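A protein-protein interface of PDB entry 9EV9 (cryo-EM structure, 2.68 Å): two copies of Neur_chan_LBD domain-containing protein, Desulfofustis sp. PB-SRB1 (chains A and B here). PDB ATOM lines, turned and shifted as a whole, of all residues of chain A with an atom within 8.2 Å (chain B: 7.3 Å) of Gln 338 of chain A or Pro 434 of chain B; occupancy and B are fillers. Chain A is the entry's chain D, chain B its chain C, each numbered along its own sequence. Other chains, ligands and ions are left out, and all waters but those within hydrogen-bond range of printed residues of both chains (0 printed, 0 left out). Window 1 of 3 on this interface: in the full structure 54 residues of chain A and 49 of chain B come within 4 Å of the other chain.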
ATOM      1  N   ALA A 335     -26.137  -7.137 -18.570  1.00  0.00           N
ATOM      2  CA  ALA A 335     -24.983  -8.022 -18.507  1.00  0.00           C
ATOM      3  C   ALA A 335     -24.640  -8.311 -17.052  1.00  0.00           C
ATOM      4  O   ALA A 335     -24.792  -7.444 -16.187  1.00  0.00           O
ATOM      5  CB  ALA A 335     -23.772  -7.410 -19.219  1.00  0.00           C
ATOM      6  N   VAL A 336     -24.178  -9.532 -16.791  1.00  0.00           N
ATOM      7  CA  VAL A 336     -23.803  -9.975 -15.453  1.00  0.00           C
ATOM      8  C   VAL A 336     -22.287 -10.082 -15.391  1.00  0.00           C
ATOM      9  O   VAL A 336     -21.668 -10.726 -16.248  1.00  0.00           O
ATOM     10  CB  VAL A 336     -24.465 -11.317 -15.095  1.00  0.00           C
ATOM     11  CG1 VAL A 336     -23.897 -11.858 -13.796  1.00  0.00           C
ATOM     12  CG2 VAL A 336     -25.971 -11.151 -14.993  1.00  0.00           C
ATOM     13  N   ASP A 337     -21.689  -9.448 -14.383  1.00  0.00           N
ATOM     14  CA  ASP A 337     -20.240  -9.427 -14.218  1.00  0.00           C
ATOM     15  C   ASP A 337     -19.742 -10.464 -13.218  1.00  0.00           C
ATOM     16  O   ASP A 337     -18.783 -11.187 -13.503  1.00  0.00           O
ATOM     17  CB  ASP A 337     -19.781  -8.028 -13.790  1.00  0.00           C
ATOM     18  CG  ASP A 337     -20.036  -6.981 -14.857  1.00  0.00           C
ATOM     19  OD1 ASP A 337     -20.027  -7.335 -16.053  1.00  0.00           O
ATOM     20  OD2 ASP A 337     -20.244  -5.803 -14.497  1.00  0.00           O
ATOM     21  N   GLN A 338     -20.372 -10.556 -12.048  1.00  0.00           N
ATOM     22  CA  GLN A 338     -19.904 -11.461 -11.010  1.00  0.00           C
ATOM     23  C   GLN A 338     -21.035 -11.756 -10.036  1.00  0.00           C
ATOM     24  O   GLN A 338     -21.758 -10.847  -9.625  1.00  0.00           O
ATOM     25  CB  GLN A 338     -18.707 -10.864 -10.257  1.00  0.00           C
ATOM     26  CG  GLN A 338     -18.248 -11.684  -9.065  1.00  0.00           C
ATOM     27  CD  GLN A 338     -17.245 -10.946  -8.201  1.00  0.00           C
ATOM     28  OE1 GLN A 338     -16.895  -9.800  -8.480  1.00  0.00           O
ATOM     29  NE2 GLN A 338     -16.779 -11.600  -7.145  1.00  0.00           N
ATOM     30  N   ILE A 339     -21.179 -13.028  -9.677  1.00  0.00           N
ATOM     31  CA  ILE A 339     -22.061 -13.440  -8.591  1.00  0.00           C
ATOM     32  C   ILE A 339     -21.258 -13.386  -7.297  1.00  0.00           C
ATOM     33  O   ILE A 339     -20.245 -14.080  -7.158  1.00  0.00           O
ATOM     34  CB  ILE A 339     -22.628 -14.846  -8.834  1.00  0.00           C
ATOM     35  CG1 ILE A 339     -23.411 -14.887 -10.148  1.00  0.00           C
ATOM     36  CG2 ILE A 339     -23.508 -15.275  -7.674  1.00  0.00           C
ATOM     37  CD1 ILE A 339     -23.976 -16.248 -10.480  1.00  0.00           C
ATOM     38  N   VAL A 340     -21.705 -12.562  -6.351  1.00  0.00           N
ATOM     39  CA  VAL A 340     -20.915 -12.241  -5.167  1.00  0.00           C
ATOM     40  C   VAL A 340     -21.434 -12.910  -3.907  1.00  0.00           C
ATOM     41  O   VAL A 340     -20.807 -12.770  -2.848  1.00  0.00           O
ATOM     42  CB  VAL A 340     -20.815 -10.718  -4.956  1.00  0.00           C
ATOM     43  CG1 VAL A 340     -20.082 -10.071  -6.118  1.00  0.00           C
ATOM     44  CG2 VAL A 340     -22.196 -10.115  -4.796  1.00  0.00           C
ATOM     45  N   GLY A 341     -22.548 -13.631  -3.976  1.00  0.00           N
ATOM     46  CA  GLY A 341     -23.030 -14.321  -2.796  1.00  0.00           C
ATOM     47  C   GLY A 341     -24.382 -14.985  -2.942  1.00  0.00           C
ATOM     48  O   GLY A 341     -25.247 -14.503  -3.677  1.00  0.00           O
ATOM     49  N   PHE A 349     -29.764 -13.937  -3.276  1.00  0.00           N
ATOM     50  CA  PHE A 349     -28.432 -13.862  -3.859  1.00  0.00           C
ATOM     51  C   PHE A 349     -28.156 -12.429  -4.290  1.00  0.00           C
ATOM     52  O   PHE A 349     -29.073 -11.624  -4.467  1.00  0.00           O
ATOM     53  CB  PHE A 349     -28.274 -14.826  -5.047  1.00  0.00           C
ATOM     54  CG  PHE A 349     -29.097 -14.455  -6.247  1.00  0.00           C
ATOM     55  CD1 PHE A 349     -30.435 -14.798  -6.320  1.00  0.00           C
ATOM     56  CD2 PHE A 349     -28.527 -13.773  -7.310  1.00  0.00           C
ATOM     57  CE1 PHE A 349     -31.193 -14.461  -7.425  1.00  0.00           C
ATOM     58  CE2 PHE A 349     -29.280 -13.434  -8.416  1.00  0.00           C
ATOM     59  CZ  PHE A 349     -30.614 -13.777  -8.474  1.00  0.00           C
ATOM     60  N   SER A 350     -26.872 -12.116  -4.456  1.00  0.00           N
ATOM     61  CA  SER A 350     -26.425 -10.784  -4.835  1.00  0.00           C
ATOM     62  C   SER A 350     -25.589 -10.863  -6.105  1.00  0.00           C
ATOM     63  O   SER A 350     -24.854 -11.832  -6.315  1.00  0.00           O
ATOM     64  CB  SER A 350     -25.613 -10.134  -3.709  1.00  0.00           C
ATOM     65  OG  SER A 350     -26.384 -10.025  -2.526  1.00  0.00           O
ATOM     66  N   VAL A 351     -25.701  -9.838  -6.950  1.00  0.00           N
ATOM     67  CA  VAL A 351     -25.071  -9.837  -8.263  1.00  0.00           C
ATOM     68  C   VAL A 351     -24.599  -8.427  -8.602  1.00  0.00           C
ATOM     69  O   VAL A 351     -25.131  -7.433  -8.098  1.00  0.00           O
ATOM     70  CB  VAL A 351     -26.035 -10.375  -9.349  1.00  0.00           C
ATOM     71  CG1 VAL A 351     -27.095  -9.340  -9.698  1.00  0.00           C
ATOM     72  CG2 VAL A 351     -25.272 -10.820 -10.585  1.00  0.00           C
ATOM     73  N   VAL A 352     -23.578  -8.350  -9.455  1.00  0.00           N
ATOM     74  CA  VAL A 352     -23.028  -7.094  -9.951  1.00  0.00           C
ATOM     75  C   VAL A 352     -23.108  -7.114 -11.472  1.00  0.00           C
ATOM     76  O   VAL A 352     -22.717  -8.103 -12.103  1.00  0.00           O
ATOM     77  CB  VAL A 352     -21.576  -6.883  -9.482  1.00  0.00           C
ATOM     78  CG1 VAL A 352     -21.022  -5.577 -10.028  1.00  0.00           C
ATOM     79  CG2 VAL A 352     -21.499  -6.905  -7.966  1.00  0.00           C
ATOM     80  N   GLY A 353     -23.607  -6.032 -12.057  1.00  0.00           N
ATOM     81  CA  GLY A 353     -23.780  -6.004 -13.494  1.00  0.00           C
ATOM     82  C   GLY A 353     -24.005  -4.602 -14.014  1.00  0.00           C
ATOM     83  O   GLY A 353     -23.790  -3.614 -13.312  1.00  0.00           O
ATOM     84  N   THR A 354     -24.445  -4.535 -15.271  1.00  0.00           N
ATOM     85  CA  THR A 354     -24.649  -3.280 -15.984  1.00  0.00           C
ATOM     86  C   THR A 354     -25.995  -3.308 -16.697  1.00  0.00           C
ATOM     87  O   THR A 354     -26.424  -4.357 -17.188  1.00  0.00           O
ATOM     88  CB  THR A 354     -23.522  -3.032 -17.000  1.00  0.00           C
ATOM     89  OG1 THR A 354     -22.253  -3.225 -16.366  1.00  0.00           O
ATOM     90  CG2 THR A 354     -23.592  -1.617 -17.547  1.00  0.00           C
ATOM     91  N   PHE A 427     -24.674  -1.433 -11.220  1.00  0.00           N
ATOM     92  CA  PHE A 427     -25.453  -1.706 -10.023  1.00  0.00           C
ATOM     93  C   PHE A 427     -24.890  -2.887  -9.248  1.00  0.00           C
ATOM     94  O   PHE A 427     -24.246  -3.778  -9.809  1.00  0.00           O
ATOM     95  CB  PHE A 427     -26.926  -1.983 -10.369  1.00  0.00           C
ATOM     96  CG  PHE A 427     -27.127  -3.158 -11.287  1.00  0.00           C
ATOM     97  CD1 PHE A 427     -27.291  -4.436 -10.778  1.00  0.00           C
ATOM     98  CD2 PHE A 427     -27.163  -2.982 -12.659  1.00  0.00           C
ATOM     99  CE1 PHE A 427     -27.477  -5.514 -11.619  1.00  0.00           C
ATOM    100  CE2 PHE A 427     -27.351  -4.056 -13.503  1.00  0.00           C
ATOM    101  CZ  PHE A 427     -27.507  -5.323 -12.982  1.00  0.00           C
ATOM    102  N   THR A 428     -25.146  -2.875  -7.941  1.00  0.00           N
ATOM    103  CA  THR A 428     -24.944  -4.023  -7.064  1.00  0.00           C
ATOM    104  C   THR A 428     -26.209  -4.182  -6.234  1.00  0.00           C
ATOM    105  O   THR A 428     -26.577  -3.268  -5.488  1.00  0.00           O
ATOM    106  CB  THR A 428     -23.723  -3.834  -6.161  1.00  0.00           C
ATOM    107  OG1 THR A 428     -22.545  -3.715  -6.967  1.00  0.00           O
ATOM    108  CG2 THR A 428     -23.568  -5.018  -5.219  1.00  0.00           C
ATOM    109  N   VAL A 429     -26.871  -5.330  -6.358  1.00  0.00           N
ATOM    110  CA  VAL A 429     -28.196  -5.518  -5.779  1.00  0.00           C
ATOM    111  C   VAL A 429     -28.316  -6.928  -5.216  1.00  0.00           C
ATOM    112  O   VAL A 429     -27.627  -7.856  -5.651  1.00  0.00           O
ATOM    113  CB  VAL A 429     -29.305  -5.239  -6.824  1.00  0.00           C
ATOM    114  CG1 VAL A 429     -29.377  -6.359  -7.853  1.00  0.00           C
ATOM    115  CG2 VAL A 429     -30.653  -5.015  -6.152  1.00  0.00           C
ATOM    116  N   VAL A 472     -23.250 -11.498 -21.861  1.00  0.00           N
ATOM    117  CA  VAL A 472     -24.225 -11.538 -20.774  1.00  0.00           C
ATOM    118  C   VAL A 472     -23.584 -12.074 -19.501  1.00  0.00           C
ATOM    119  O   VAL A 472     -23.802 -11.541 -18.406  1.00  0.00           O
ATOM    120  CB  VAL A 472     -25.453 -12.366 -21.191  1.00  0.00           C
ATOM    121  CG1 VAL A 472     -26.451 -12.448 -20.049  1.00  0.00           C
ATOM    122  CG2 VAL A 472     -26.100 -11.759 -22.423  1.00  0.00           C
ATOM    123  N   VAL A 473     -22.778 -13.125 -19.621  1.00  0.00           N
ATOM    124  CA  VAL A 473     -22.045 -13.696 -18.497  1.00  0.00           C
ATOM    125  C   VAL A 473     -20.559 -13.458 -18.738  1.00  0.00           C
ATOM    126  O   VAL A 473     -20.014 -13.873 -19.768  1.00  0.00           O
ATOM    127  CB  VAL A 473     -22.356 -15.189 -18.313  1.00  0.00           C
ATOM    128  CG1 VAL A 473     -22.385 -15.905 -19.658  1.00  0.00           C
ATOM    129  CG2 VAL A 473     -21.342 -15.834 -17.381  1.00  0.00           C
ATOM    130  N   GLY A 474     -19.910 -12.780 -17.795  1.00  0.00           N
ATOM    131  CA  GLY A 474     -18.511 -12.418 -17.945  1.00  0.00           C
ATOM    132  C   GLY A 474     -17.586 -13.435 -17.297  1.00  0.00           C
ATOM    133  O   GLY A 474     -17.936 -14.080 -16.311  1.00  0.00           O
ATOM    134  N   ASP A 475     -16.393 -13.568 -17.873  1.00  0.00           N
ATOM    135  CA  ASP A 475     -15.378 -14.474 -17.353  1.00  0.00           C
ATOM    136  C   ASP A 475     -14.462 -13.739 -16.386  1.00  0.00           C
ATOM    137  O   ASP A 475     -14.121 -12.572 -16.597  1.00  0.00           O
ATOM    138  CB  ASP A 475     -14.560 -15.079 -18.495  1.00  0.00           C
ATOM    139  CG  ASP A 475     -13.865 -14.026 -19.338  1.00  0.00           C
ATOM    140  OD1 ASP A 475     -14.422 -12.919 -19.487  1.00  0.00           O
ATOM    141  OD2 ASP A 475     -12.762 -14.308 -19.852  1.00  0.00           O
ATOM    142  N   GLN A 476     -14.066 -14.430 -15.319  1.00  0.00           N
ATOM    143  CA  GLN A 476     -13.177 -13.876 -14.310  1.00  0.00           C
ATOM    144  C   GLN A 476     -12.078 -14.879 -13.993  1.00  0.00           C
ATOM    145  O   GLN A 476     -12.259 -16.091 -14.139  1.00  0.00           O
ATOM    146  CB  GLN A 476     -13.935 -13.508 -13.024  1.00  0.00           C
ATOM    147  CG  GLN A 476     -15.054 -12.492 -13.218  1.00  0.00           C
ATOM    148  CD  GLN A 476     -14.544 -11.111 -13.587  1.00  0.00           C
ATOM    149  OE1 GLN A 476     -13.353 -10.820 -13.465  1.00  0.00           O
ATOM    150  NE2 GLN A 476     -15.447 -10.249 -14.041  1.00  0.00           N
ATOM    151  N   LEU A 477     -10.932 -14.359 -13.560  1.00  0.00           N
ATOM    152  CA  LEU A 477      -9.804 -15.211 -13.214  1.00  0.00           C
ATOM    153  C   LEU A 477     -10.115 -16.039 -11.972  1.00  0.00           C
ATOM    154  O   LEU A 477     -10.820 -15.598 -11.060  1.00  0.00           O
ATOM    155  CB  LEU A 477      -8.549 -14.370 -12.981  1.00  0.00           C
ATOM    156  CG  LEU A 477      -8.037 -13.566 -14.175  1.00  0.00           C
ATOM    157  CD1 LEU A 477      -6.791 -12.778 -13.798  1.00  0.00           C
ATOM    158  CD2 LEU A 477      -7.760 -14.478 -15.360  1.00  0.00           C
ATOM    159  N   GLY A 478      -9.576 -17.256 -11.943  1.00  0.00           N
ATOM    160  CA  GLY A 478      -9.793 -18.159 -10.832  1.00  0.00           C
ATOM    161  C   GLY A 478     -11.056 -18.981 -10.983  1.00  0.00           C
ATOM    162  O   GLY A 478     -11.845 -18.829 -11.920  1.00  0.00           O
ATOM    163  N   GLU A 479     -11.248 -19.878 -10.023  1.00  0.00           N
ATOM    164  CA  GLU A 479     -12.409 -20.754 -10.009  1.00  0.00           C
ATOM    165  C   GLU A 479     -13.573 -20.089  -9.282  1.00  0.00           C
ATOM    166  O   GLU A 479     -13.400 -19.135  -8.519  1.00  0.00           O
ATOM    167  CB  GLU A 479     -12.070 -22.091  -9.349  1.00  0.00           C
ATOM    168  CG  GLU A 479     -10.934 -22.847 -10.017  1.00  0.00           C
ATOM    169  CD  GLU A 479     -11.282 -23.320 -11.417  1.00  0.00           C
ATOM    170  OE1 GLU A 479     -12.485 -23.482 -11.713  1.00  0.00           O
ATOM    171  OE2 GLU A 479     -10.352 -23.527 -12.222  1.00  0.00           O
ATOM    172  N   GLU A 480     -14.770 -20.611  -9.529  1.00  0.00           N
ATOM    173  CA  GLU A 480     -15.987 -20.091  -8.927  1.00  0.00           C
ATOM    174  C   GLU A 480     -16.747 -21.218  -8.244  1.00  0.00           C
ATOM    175  O   GLU A 480     -16.703 -22.374  -8.667  1.00  0.00           O
ATOM    176  CB  GLU A 480     -16.888 -19.405  -9.966  1.00  0.00           C
ATOM    177  CG  GLU A 480     -16.443 -18.004 -10.367  1.00  0.00           C
ATOM    178  CD  GLU A 480     -15.211 -18.003 -11.252  1.00  0.00           C
ATOM    179  OE1 GLU A 480     -14.920 -19.047 -11.872  1.00  0.00           O
ATOM    180  OE2 GLU A 480     -14.534 -16.956 -11.328  1.00  0.00           O
ATOM    181  N   LEU A 509     -30.262 -17.353 -15.312  1.00  0.00           N
ATOM    182  CA  LEU A 509     -28.987 -18.060 -15.302  1.00  0.00           C
ATOM    183  C   LEU A 509     -29.182 -19.439 -14.687  1.00  0.00           C
ATOM    184  O   LEU A 509     -29.783 -19.564 -13.615  1.00  0.00           O
ATOM    185  CB  LEU A 509     -27.929 -17.281 -14.517  1.00  0.00           C
ATOM    186  CG  LEU A 509     -27.641 -15.840 -14.936  1.00  0.00           C
ATOM    187  CD1 LEU A 509     -26.591 -15.219 -14.029  1.00  0.00           C
ATOM    188  CD2 LEU A 509     -27.199 -15.780 -16.384  1.00  0.00           C
ATOM    189  N   ARG B 345     -14.128 -14.877   0.153  1.00  0.00           N
ATOM    190  CA  ARG B 345     -15.312 -15.448  -0.478  1.00  0.00           C
ATOM    191  C   ARG B 345     -16.018 -14.449  -1.384  1.00  0.00           C
ATOM    192  O   ARG B 345     -16.401 -14.797  -2.507  1.00  0.00           O
ATOM    193  CB  ARG B 345     -16.286 -15.965   0.584  1.00  0.00           C
ATOM    194  CG  ARG B 345     -15.873 -17.282   1.211  1.00  0.00           C
ATOM    195  CD  ARG B 345     -16.968 -17.826   2.112  1.00  0.00           C
ATOM    196  NE  ARG B 345     -18.229 -17.986   1.398  1.00  0.00           N
ATOM    197  CZ  ARG B 345     -18.585 -19.081   0.739  1.00  0.00           C
ATOM    198  NH1 ARG B 345     -17.795 -20.140   0.680  1.00  0.00           N
ATOM    199  NH2 ARG B 345     -19.764 -19.113   0.126  1.00  0.00           N
ATOM    200  N   SER B 346     -16.197 -13.213  -0.922  1.00  0.00           N
ATOM    201  CA  SER B 346     -16.814 -12.170  -1.729  1.00  0.00           C
ATOM    202  C   SER B 346     -15.817 -11.442  -2.621  1.00  0.00           C
ATOM    203  O   SER B 346     -16.233 -10.615  -3.440  1.00  0.00           O
ATOM    204  CB  SER B 346     -17.528 -11.160  -0.825  1.00  0.00           C
ATOM    205  OG  SER B 346     -18.115 -10.119  -1.586  1.00  0.00           O
ATOM    206  N   GLU B 347     -14.522 -11.732  -2.479  1.00  0.00           N
ATOM    207  CA  GLU B 347     -13.468 -11.190  -3.338  1.00  0.00           C
ATOM    208  C   GLU B 347     -13.446  -9.659  -3.310  1.00  0.00           C
ATOM    209  O   GLU B 347     -13.681  -8.985  -4.315  1.00  0.00           O
ATOM    210  CB  GLU B 347     -13.602 -11.721  -4.768  1.00  0.00           C
ATOM    211  CG  GLU B 347     -13.406 -13.223  -4.886  1.00  0.00           C
ATOM    212  CD  GLU B 347     -13.302 -13.688  -6.324  1.00  0.00           C
ATOM    213  OE1 GLU B 347     -13.243 -12.828  -7.227  1.00  0.00           O
ATOM    214  OE2 GLU B 347     -13.278 -14.917  -6.551  1.00  0.00           O
ATOM    215  N   ASN B 348     -13.161  -9.120  -2.128  1.00  0.00           N
ATOM    216  CA  ASN B 348     -12.971  -7.687  -1.966  1.00  0.00           C
ATOM    217  C   ASN B 348     -11.992  -7.441  -0.827  1.00  0.00           C
ATOM    218  O   ASN B 348     -11.779  -8.301   0.031  1.00  0.00           O
ATOM    219  CB  ASN B 348     -14.297  -6.960  -1.706  1.00  0.00           C
ATOM    220  CG  ASN B 348     -14.992  -7.442  -0.449  1.00  0.00           C
ATOM    221  OD1 ASN B 348     -14.646  -7.040   0.661  1.00  0.00           O
ATOM    222  ND2 ASN B 348     -15.989  -8.298  -0.619  1.00  0.00           N
ATOM    223  N   ASN B 401     -13.987   0.537  -8.541  1.00  0.00           N
ATOM    224  CA  ASN B 401     -14.501  -0.678  -7.923  1.00  0.00           C
ATOM    225  C   ASN B 401     -14.969  -0.445  -6.489  1.00  0.00           C
ATOM    226  O   ASN B 401     -14.845  -1.331  -5.640  1.00  0.00           O
ATOM    227  CB  ASN B 401     -13.447  -1.784  -7.962  1.00  0.00           C
ATOM    228  CG  ASN B 401     -13.025  -2.136  -9.372  1.00  0.00           C
ATOM    229  OD1 ASN B 401     -13.677  -2.931 -10.048  1.00  0.00           O
ATOM    230  ND2 ASN B 401     -11.924  -1.547  -9.825  1.00  0.00           N
ATOM    231  N   LEU B 431     -12.908  -2.163  -1.872  1.00  0.00           N
ATOM    232  CA  LEU B 431     -12.818  -2.301  -3.318  1.00  0.00           C
ATOM    233  C   LEU B 431     -12.977  -3.758  -3.724  1.00  0.00           C
ATOM    234  O   LEU B 431     -12.411  -4.656  -3.092  1.00  0.00           O
ATOM    235  CB  LEU B 431     -11.482  -1.764  -3.837  1.00  0.00           C
ATOM    236  CG  LEU B 431     -11.147  -0.315  -3.483  1.00  0.00           C
ATOM    237  CD1 LEU B 431      -9.782   0.066  -4.029  1.00  0.00           C
ATOM    238  CD2 LEU B 431     -12.217   0.628  -4.003  1.00  0.00           C
ATOM    239  N   GLN B 432     -13.748  -3.985  -4.786  1.00  0.00           N
ATOM    240  CA  GLN B 432     -13.930  -5.329  -5.317  1.00  0.00           C
ATOM    241  C   GLN B 432     -12.698  -5.770  -6.101  1.00  0.00           C
ATOM    242  O   GLN B 432     -12.039  -4.971  -6.771  1.00  0.00           O
ATOM    243  CB  GLN B 432     -15.167  -5.383  -6.210  1.00  0.00           C
ATOM    244  CG  GLN B 432     -16.444  -4.931  -5.519  1.00  0.00           C
ATOM    245  CD  GLN B 432     -17.637  -4.910  -6.453  1.00  0.00           C
ATOM    246  OE1 GLN B 432     -17.527  -5.272  -7.624  1.00  0.00           O
ATOM    247  NE2 GLN B 432     -18.784  -4.483  -5.939  1.00  0.00           N
ATOM    248  N   ALA B 433     -12.390  -7.060  -6.010  1.00  0.00           N
ATOM    249  CA  ALA B 433     -11.221  -7.646  -6.667  1.00  0.00           C
ATOM    250  C   ALA B 433     -11.621  -8.950  -7.343  1.00  0.00           C
ATOM    251  O   ALA B 433     -11.391 -10.042  -6.815  1.00  0.00           O
ATOM    252  CB  ALA B 433     -10.088  -7.869  -5.665  1.00  0.00           C
ATOM    253  N   PRO B 434     -12.231  -8.868  -8.530  1.00  0.00           N
ATOM    254  CA  PRO B 434     -12.643 -10.096  -9.232  1.00  0.00           C
ATOM    255  C   PRO B 434     -11.483 -10.922  -9.765  1.00  0.00           C
ATOM    256  O   PRO B 434     -11.710 -12.060 -10.198  1.00  0.00           O
ATOM    257  CB  PRO B 434     -13.515  -9.565 -10.376  1.00  0.00           C
ATOM    258  CG  PRO B 434     -13.000  -8.188 -10.623  1.00  0.00           C
ATOM    259  CD  PRO B 434     -12.585  -7.653  -9.282  1.00  0.00           C
ATOM    260  N   ASP B 435     -10.257 -10.397  -9.754  1.00  0.00           N
ATOM    261  CA  ASP B 435      -9.109 -11.110 -10.299  1.00  0.00           C
ATOM    262  C   ASP B 435      -8.430 -12.024  -9.286  1.00  0.00           C
ATOM    263  O   ASP B 435      -7.398 -12.619  -9.617  1.00  0.00           O
ATOM    264  CB  ASP B 435      -8.089 -10.114 -10.851  1.00  0.00           C
ATOM    265  CG  ASP B 435      -8.662  -9.239 -11.947  1.00  0.00           C
ATOM    266  OD1 ASP B 435      -9.854  -9.406 -12.280  1.00  0.00           O
ATOM    267  OD2 ASP B 435      -7.923  -8.380 -12.473  1.00  0.00           O
ATOM    268  N   PHE B 436      -8.966 -12.142  -8.073  1.00  0.00           N
ATOM    269  CA  PHE B 436      -8.362 -13.004  -7.064  1.00  0.00           C
ATOM    270  C   PHE B 436      -8.318 -14.452  -7.538  1.00  0.00           C
ATOM    271  O   PHE B 436      -9.241 -14.938  -8.196  1.00  0.00           O
ATOM    272  CB  PHE B 436      -9.140 -12.914  -5.751  1.00  0.00           C
ATOM    273  CG  PHE B 436      -8.778 -11.727  -4.907  1.00  0.00           C
ATOM    274  CD1 PHE B 436      -7.634 -10.993  -5.167  1.00  0.00           C
ATOM    275  CD2 PHE B 436      -9.579 -11.354  -3.840  1.00  0.00           C
ATOM    276  CE1 PHE B 436      -7.301  -9.905  -4.385  1.00  0.00           C
ATOM    277  CE2 PHE B 436      -9.250 -10.268  -3.056  1.00  0.00           C
ATOM    278  CZ  PHE B 436      -8.111  -9.545  -3.327  1.00  0.00           C
ATOM    279  N   ASP B 437      -7.229 -15.139  -7.199  1.00  0.00           N
ATOM    280  CA  ASP B 437      -7.037 -16.543  -7.555  1.00  0.00           C
ATOM    281  C   ASP B 437      -6.394 -17.244  -6.366  1.00  0.00           C
ATOM    282  O   ASP B 437      -5.220 -17.007  -6.067  1.00  0.00           O
ATOM    283  CB  ASP B 437      -6.174 -16.682  -8.809  1.00  0.00           C
ATOM    284  CG  ASP B 437      -6.123 -18.105  -9.331  1.00  0.00           C
ATOM    285  OD1 ASP B 437      -6.872 -18.961  -8.815  1.00  0.00           O
ATOM    286  OD2 ASP B 437      -5.329 -18.369 -10.259  1.00  0.00           O
ATOM    287  N   SER B 449      -5.250  -3.784  -6.764  1.00  0.00           N
ATOM    288  CA  SER B 449      -5.298  -2.701  -7.735  1.00  0.00           C
ATOM    289  C   SER B 449      -6.262  -1.620  -7.261  1.00  0.00           C
ATOM    290  O   SER B 449      -7.404  -1.916  -6.898  1.00  0.00           O
ATOM    291  CB  SER B 449      -5.721  -3.221  -9.110  1.00  0.00           C
ATOM    292  OG  SER B 449      -7.001  -3.826  -9.054  1.00  0.00           O
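No position is printed for both chains.
Of the 11 pairs that touch across the chains among the printed residues, none has its exchanged pair printed and touching as well.
Of chain B, only Ser 346 (3.9 Å), Glu 347 (3.7 Å) and Pro 434 (3.9 Å) come within 4 Å of Gln 338 of chain A.
Of chain A, only Gln 338 (3.9 Å), Gln 476 (3.3 Å) and Leu 477 (3.7 Å) come within 4 Å of Pro 434 of chain B.
No residue of chain A comes within 4 Å of Ala 433 of chain B.
Printed residues of chain B within 4 Å of Val 340 of chain A: Ser 346.
Printed residues of chain B within 4 Å of Gln 476 of chain A: Pro 434 (3.3 Å) and Asp 435 (3.96 Å).
Of the printed residues of chain A, Gln 432 of chain B touches Thr 428 (3.97 Å).
Of the printed residues of chain B, Thr 428 of chain A touches Gln 432 (3.97 Å).
Ile 339 of chain A touches none of the printed residues of chain B.
Gly 353 of chain A touches none of the printed residues of chain B.
The nearest printed residue of chain A that does not touch Phe 436 of chain B is Gly 478 of chain A (4.2 Å).
O of Leu 477 of chain A sits close to O of Phe 436 of chain B (3.3 Å).
Gln 338 of chain A touches Ser 346 of chain B.
Gln 338 of chain A touches Glu 347 of chain B (NE2 to OE1, 3.7 Å).
Pro 434 of chain B touches Gln 338 of chain A.
Val 340 of chain A touches Ser 346 of chain B (O to OG, 3.98 Å).
Thr 428 of chain A touches Gln 432 of chain B (OG1 to NE2, 3.97 Å).
Pro 434 of chain B touches Gln 476 of chain A.
Gln 476 of chain A touches Asp 435 of chain B (OE1 to OD1, 3.96 Å).
O of Pro 434 of chain B touches O of Leu 477 of chain A, 3.7 Å away.
O of Asp 435 of chain B touches CB of Leu 477 of chain A, at 3.96 Å.
Gly 478 of chain A touches Asp 437 of chain B (CA to OD1, 3.6 Å).
The side-chain hydroxyl (OG) of Ser 346 of chain B sits at hydrogen-bond distance from the side-chain amide nitrogen (ND2) of Asn 348 of chain B, at 3.0 Å.
The backbone carbonyl oxygen (O) of Glu 347 of chain B sits at hydrogen-bond distance from the backbone NH (N) of Ala 433 of chain B (2.9 Å).
The backbone NH (N) of Gln 432 of chain B lies within hydrogen-bond range of the backbone carbonyl oxygen (O) of Asn 401 of chain B.
O of Gln 338 of chain A lies within hydrogen-bond range of N of Val 352 of chain A.
The backbone carbonyl oxygen (O) of Ser 350 of chain A sits at hydrogen-bond distance from the backbone NH (N) of Val 340 of chain A (3.2 Å).
Of the 26 printed residues of chain A, 6 touch a printed residue of chain B.
Of the 13 printed residues of chain B, 7 touch a printed residue of chain A.
Hydrophobic or aromatic side chains of chain B within 4 Å of the printed part of chain A: Pro 434.
Among the printed residues, no Asp or Glu carboxylate lies within 4 Å of a Lys or Arg side-chain nitrogen of the other chain.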
